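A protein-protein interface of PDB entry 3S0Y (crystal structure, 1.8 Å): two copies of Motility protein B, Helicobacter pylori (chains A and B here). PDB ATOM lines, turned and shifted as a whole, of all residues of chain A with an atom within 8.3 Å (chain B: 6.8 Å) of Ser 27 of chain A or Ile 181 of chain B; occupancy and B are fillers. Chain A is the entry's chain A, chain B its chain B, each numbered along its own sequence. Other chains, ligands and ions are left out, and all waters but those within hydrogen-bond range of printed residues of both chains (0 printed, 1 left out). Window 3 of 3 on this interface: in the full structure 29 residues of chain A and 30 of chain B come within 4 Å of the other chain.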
ATOM      1  N   SER A  23      -9.367 -34.368   9.556  1.00  0.00           N
ATOM      2  CA  SER A  23     -10.403 -33.484  10.084  1.00  0.00           C
ATOM      3  C   SER A  23      -9.818 -32.128  10.480  1.00  0.00           C
ATOM      4  O   SER A  23      -8.607 -31.912  10.384  1.00  0.00           O
ATOM      5  CB  SER A  23     -11.092 -34.132  11.288  1.00  0.00           C
ATOM      6  N   LYS A  24     -10.686 -31.219  10.919  1.00  0.00           N
ATOM      7  CA  LYS A  24     -10.261 -29.881  11.321  1.00  0.00           C
ATOM      8  C   LYS A  24      -9.344 -29.946  12.551  1.00  0.00           C
ATOM      9  O   LYS A  24      -9.657 -30.660  13.509  1.00  0.00           O
ATOM     10  CB  LYS A  24     -11.483 -29.008  11.637  1.00  0.00           C
ATOM     11  N   PRO A  25      -8.196 -29.231  12.516  1.00  0.00           N
ATOM     12  CA  PRO A  25      -7.358 -29.048  13.709  1.00  0.00           C
ATOM     13  C   PRO A  25      -8.142 -28.655  14.966  1.00  0.00           C
ATOM     14  O   PRO A  25      -7.910 -29.216  16.039  1.00  0.00           O
ATOM     15  CB  PRO A  25      -6.417 -27.915  13.297  1.00  0.00           C
ATOM     16  CG  PRO A  25      -6.230 -28.099  11.809  1.00  0.00           C
ATOM     17  CD  PRO A  25      -7.486 -28.808  11.291  1.00  0.00           C
ATOM     18  N   ALA A  26      -9.052 -27.694  14.822  1.00  0.00           N
ATOM     19  CA  ALA A  26      -9.935 -27.288  15.911  1.00  0.00           C
ATOM     20  C   ALA A  26     -11.306 -27.937  15.748  1.00  0.00           C
ATOM     21  O   ALA A  26     -12.222 -27.343  15.155  1.00  0.00           O
ATOM     22  CB  ALA A  26     -10.065 -25.786  15.941  1.00  0.00           C
ATOM     23  N   SER A  27     -11.441 -29.153  16.287  1.00  0.00           N
ATOM     24  CA  SER A  27     -12.674 -29.944  16.150  1.00  0.00           C
ATOM     25  C   SER A  27     -13.611 -29.716  17.346  1.00  0.00           C
ATOM     26  O   SER A  27     -13.507 -30.399  18.373  1.00  0.00           O
ATOM     27  CB  SER A  27     -12.333 -31.442  15.996  1.00  0.00           C
ATOM     28  OG  SER A  27     -13.483 -32.227  15.695  1.00  0.00           O
ATOM     29  N   GLN A  28     -14.516 -28.745  17.210  1.00  0.00           N
ATOM     30  CA  GLN A  28     -15.521 -28.478  18.236  1.00  0.00           C
ATOM     31  C   GLN A  28     -16.842 -29.115  17.844  1.00  0.00           C
ATOM     32  O   GLN A  28     -17.190 -29.153  16.654  1.00  0.00           O
ATOM     33  CB  GLN A  28     -15.728 -26.984  18.417  1.00  0.00           C
ATOM     34  N   ASN A  29     -17.567 -29.610  18.844  1.00  0.00           N
ATOM     35  CA  ASN A  29     -18.835 -30.300  18.615  1.00  0.00           C
ATOM     36  C   ASN A  29     -19.988 -29.623  19.357  1.00  0.00           C
ATOM     37  O   ASN A  29     -20.112 -29.725  20.576  1.00  0.00           O
ATOM     38  CB  ASN A  29     -18.744 -31.758  19.038  1.00  0.00           C
ATOM     39  CG  ASN A  29     -20.085 -32.444  18.995  1.00  0.00           C
ATOM     40  OD1 ASN A  29     -20.866 -32.240  18.059  1.00  0.00           O
ATOM     41  ND2 ASN A  29     -20.376 -33.250  20.017  1.00  0.00           N
ATOM     42  N   THR A  30     -20.853 -28.970  18.593  1.00  0.00           N
ATOM     43  CA  THR A  30     -21.907 -28.151  19.159  1.00  0.00           C
ATOM     44  C   THR A  30     -23.249 -28.881  19.209  1.00  0.00           C
ATOM     45  O   THR A  30     -24.297 -28.240  19.368  1.00  0.00           O
ATOM     46  CB  THR A  30     -22.046 -26.897  18.341  1.00  0.00           C
ATOM     47  OG1 THR A  30     -22.290 -27.268  16.982  1.00  0.00           O
ATOM     48  CG2 THR A  30     -20.762 -26.083  18.420  1.00  0.00           C
ATOM     49  N   SER B 176     -20.031 -21.037  19.789  1.00  0.00           N
ATOM     50  CA  SER B 176     -20.530 -22.277  20.337  1.00  0.00           C
ATOM     51  C   SER B 176     -19.472 -23.370  20.301  1.00  0.00           C
ATOM     52  O   SER B 176     -19.336 -24.134  21.262  1.00  0.00           O
ATOM     53  CB  SER B 176     -21.786 -22.720  19.571  1.00  0.00           C
ATOM     54  OG  SER B 176     -22.802 -21.725  19.692  1.00  0.00           O
ATOM     55  N   LYS B 177     -18.729 -23.447  19.200  1.00  0.00           N
ATOM     56  CA  LYS B 177     -17.645 -24.430  19.042  1.00  0.00           C
ATOM     57  C   LYS B 177     -16.525 -24.141  20.040  1.00  0.00           C
ATOM     58  O   LYS B 177     -16.005 -25.051  20.679  1.00  0.00           O
ATOM     59  CB  LYS B 177     -17.091 -24.396  17.609  1.00  0.00           C
ATOM     60  CG  LYS B 177     -17.977 -25.055  16.566  1.00  0.00           C
ATOM     61  CD  LYS B 177     -17.327 -24.925  15.176  1.00  0.00           C
ATOM     62  CE  LYS B 177     -18.199 -25.446  14.051  1.00  0.00           C
ATOM     63  NZ  LYS B 177     -17.367 -25.851  12.863  1.00  0.00           N
ATOM     64  N   ILE B 178     -16.185 -22.862  20.198  1.00  0.00           N
ATOM     65  CA  ILE B 178     -15.166 -22.461  21.151  1.00  0.00           C
ATOM     66  C   ILE B 178     -15.551 -22.951  22.534  1.00  0.00           C
ATOM     67  O   ILE B 178     -14.773 -23.620  23.212  1.00  0.00           O
ATOM     68  CB  ILE B 178     -14.993 -20.942  21.182  1.00  0.00           C
ATOM     69  CG1 ILE B 178     -14.360 -20.457  19.891  1.00  0.00           C
ATOM     70  CG2 ILE B 178     -14.131 -20.498  22.384  1.00  0.00           C
ATOM     71  CD1 ILE B 178     -14.363 -18.915  19.791  1.00  0.00           C
ATOM     72  N   HIS B 179     -16.772 -22.647  22.945  1.00  0.00           N
ATOM     73  CA  HIS B 179     -17.187 -23.070  24.253  1.00  0.00           C
ATOM     74  C   HIS B 179     -17.181 -24.602  24.441  1.00  0.00           C
ATOM     75  O   HIS B 179     -16.797 -25.084  25.483  1.00  0.00           O
ATOM     76  CB  HIS B 179     -18.541 -22.497  24.605  1.00  0.00           C
ATOM     77  CG  HIS B 179     -18.857 -22.672  26.038  1.00  0.00           C
ATOM     78  ND1 HIS B 179     -18.264 -21.902  27.017  1.00  0.00           N
ATOM     79  CD2 HIS B 179     -19.613 -23.592  26.676  1.00  0.00           C
ATOM     80  CE1 HIS B 179     -18.688 -22.312  28.195  1.00  0.00           C
ATOM     81  NE2 HIS B 179     -19.513 -23.325  28.016  1.00  0.00           N
ATOM     82  N   SER B 180     -17.618 -25.342  23.439  1.00  0.00           N
ATOM     83  CA  SER B 180     -17.662 -26.812  23.521  1.00  0.00           C
ATOM     84  C   SER B 180     -16.264 -27.379  23.731  1.00  0.00           C
ATOM     85  O   SER B 180     -16.052 -28.263  24.568  1.00  0.00           O
ATOM     86  CB  SER B 180     -18.270 -27.391  22.243  1.00  0.00           C
ATOM     87  OG  SER B 180     -18.249 -28.824  22.250  1.00  0.00           O
ATOM     88  N   ILE B 181     -15.304 -26.839  22.993  1.00  0.00           N
ATOM     89  CA  ILE B 181     -13.909 -27.272  23.109  1.00  0.00           C
ATOM     90  C   ILE B 181     -13.349 -26.981  24.495  1.00  0.00           C
ATOM     91  O   ILE B 181     -12.786 -27.868  25.119  1.00  0.00           O
ATOM     92  CB  ILE B 181     -13.031 -26.619  22.041  1.00  0.00           C
ATOM     93  CG1 ILE B 181     -13.430 -27.140  20.661  1.00  0.00           C
ATOM     94  CG2 ILE B 181     -11.544 -26.948  22.274  1.00  0.00           C
ATOM     95  CD1 ILE B 181     -12.857 -26.342  19.518  1.00  0.00           C
ATOM     96  N   LEU B 182     -13.523 -25.751  24.972  1.00  0.00           N
ATOM     97  CA  LEU B 182     -13.078 -25.395  26.318  1.00  0.00           C
ATOM     98  C   LEU B 182     -13.761 -26.255  27.394  1.00  0.00           C
ATOM     99  O   LEU B 182     -13.101 -26.690  28.349  1.00  0.00           O
ATOM    100  CB  LEU B 182     -13.335 -23.901  26.595  1.00  0.00           C
ATOM    101  CG  LEU B 182     -12.497 -22.887  25.798  1.00  0.00           C
ATOM    102  CD1 LEU B 182     -12.946 -21.429  26.027  1.00  0.00           C
ATOM    103  CD2 LEU B 182     -10.995 -23.050  26.097  1.00  0.00           C
ATOM    104  N   ASP B 183     -15.069 -26.482  27.241  1.00  0.00           N
ATOM    105  CA  ASP B 183     -15.838 -27.261  28.217  1.00  0.00           C
ATOM    106  C   ASP B 183     -15.344 -28.725  28.275  1.00  0.00           C
ATOM    107  O   ASP B 183     -15.177 -29.298  29.378  1.00  0.00           O
ATOM    108  CB  ASP B 183     -17.333 -27.213  27.886  1.00  0.00           C
ATOM    109  CG  ASP B 183     -18.183 -28.000  28.881  1.00  0.00           C
ATOM    110  OD1 ASP B 183     -18.287 -27.573  30.047  1.00  0.00           O
ATOM    111  OD2 ASP B 183     -18.726 -29.072  28.503  1.00  0.00           O
ATOM    112  N   ASN B 184     -15.127 -29.313  27.103  1.00  0.00           N
ATOM    113  CA  ASN B 184     -14.600 -30.679  26.984  1.00  0.00           C
ATOM    114  C   ASN B 184     -13.198 -30.825  27.573  1.00  0.00           C
ATOM    115  O   ASN B 184     -12.873 -31.855  28.138  1.00  0.00           O
ATOM    116  CB  ASN B 184     -14.583 -31.123  25.517  1.00  0.00           C
ATOM    117  CG  ASN B 184     -15.953 -31.561  25.020  1.00  0.00           C
ATOM    118  OD1 ASN B 184     -16.633 -32.359  25.671  1.00  0.00           O
ATOM    119  ND2 ASN B 184     -16.350 -31.068  23.845  1.00  0.00           N
ATOM    120  N   GLU B 185     -12.364 -29.797  27.420  1.00  0.00           N
ATOM    121  CA  GLU B 185     -11.015 -29.825  27.979  1.00  0.00           C
ATOM    122  C   GLU B 185     -10.961 -29.587  29.481  1.00  0.00           C
ATOM    123  O   GLU B 185     -10.100 -30.147  30.138  1.00  0.00           O
ATOM    124  CB  GLU B 185     -10.127 -28.788  27.302  1.00  0.00           C
ATOM    125  CG  GLU B 185      -9.788 -29.129  25.877  1.00  0.00           C
ATOM    126  CD  GLU B 185      -8.851 -30.309  25.768  1.00  0.00           C
ATOM    127  OE1 GLU B 185      -7.881 -30.367  26.556  1.00  0.00           O
ATOM    128  OE2 GLU B 185      -9.089 -31.174  24.894  1.00  0.00           O
ATOM    129  N   PHE B 186     -11.836 -28.730  30.009  1.00  0.00           N
ATOM    130  CA  PHE B 186     -11.740 -28.287  31.417  1.00  0.00           C
ATOM    131  C   PHE B 186     -12.853 -28.815  32.327  1.00  0.00           C
ATOM    132  O   PHE B 186     -12.624 -29.027  33.518  1.00  0.00           O
ATOM    133  CB  PHE B 186     -11.754 -26.759  31.511  1.00  0.00           C
ATOM    134  CG  PHE B 186     -10.559 -26.089  30.884  1.00  0.00           C
ATOM    135  CD1 PHE B 186      -9.282 -26.389  31.303  1.00  0.00           C
ATOM    136  CD2 PHE B 186     -10.728 -25.129  29.894  1.00  0.00           C
ATOM    137  CE1 PHE B 186      -8.182 -25.761  30.726  1.00  0.00           C
ATOM    138  CE2 PHE B 186      -9.635 -24.492  29.325  1.00  0.00           C
ATOM    139  CZ  PHE B 186      -8.365 -24.812  29.740  1.00  0.00           C
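Of the printed residues of chain B, Ser 27 of chain A touches Ile 181. Of the printed residues of chain B, Gln 28 of chain A touches Lys 177 (3.0 Å) and Ile 181 (3.1 Å). Of the printed residues of chain B, Asn 29 of chain A touches Ser 180 (2.7 Å). Of the printed residues of chain B, Thr 30 of chain A touches Ser 176 (3.5 Å) and Lys 177 (3.4 Å). Of chain A, only Asn 29 (2.7 Å) comes within 4 Å of Ser 180 of chain B. Of the printed residues of chain A, Ile 181 of chain B touches Ser 27 (3.98 Å) and Gln 28 (3.1 Å). Asn 184 of chain B touches none of the printed residues of chain A.
Of the 8 printed residues of chain A, 4 touch a printed residue of chain B. Of the 11 printed residues of chain B, 4 touch a printed residue of chain A. Hydrophobic or aromatic side chains of chain B that line the printed part of chain A: Ile 181. Among the printed residues, 6 pairs touch across the chains.
Among the printed residues, merely in contact across the chains: Gln 28 of chain A with Lys 177 of chain B (3.0 Å), Gln 28 of chain A with Ile 181 of chain B (3.1 Å), Thr 30 of chain A with Lys 177 of chain B (3.4 Å), Thr 30 of chain A with Ser 176 of chain B (3.5 Å) and Ser 27 of chain A with Ile 181 of chain B (3.98 Å).
The backbone carbonyl oxygen (O) of Ser 180 of chain B lies within hydrogen-bond range of the side-chain amide nitrogen (ND2) of Asn 184 of chain B, 2.9 Å away.
No position is printed for both chains. Of the 6 pairs that touch across the chains among the printed residues, none has its exchanged pair printed and touching as well.
The backbone carbonyl oxygen (O) of Asn 29 of chain A is in hydrogen-bond range of the side-chain hydroxyl (OG) of Ser 180 of chain B (2.7 Å).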
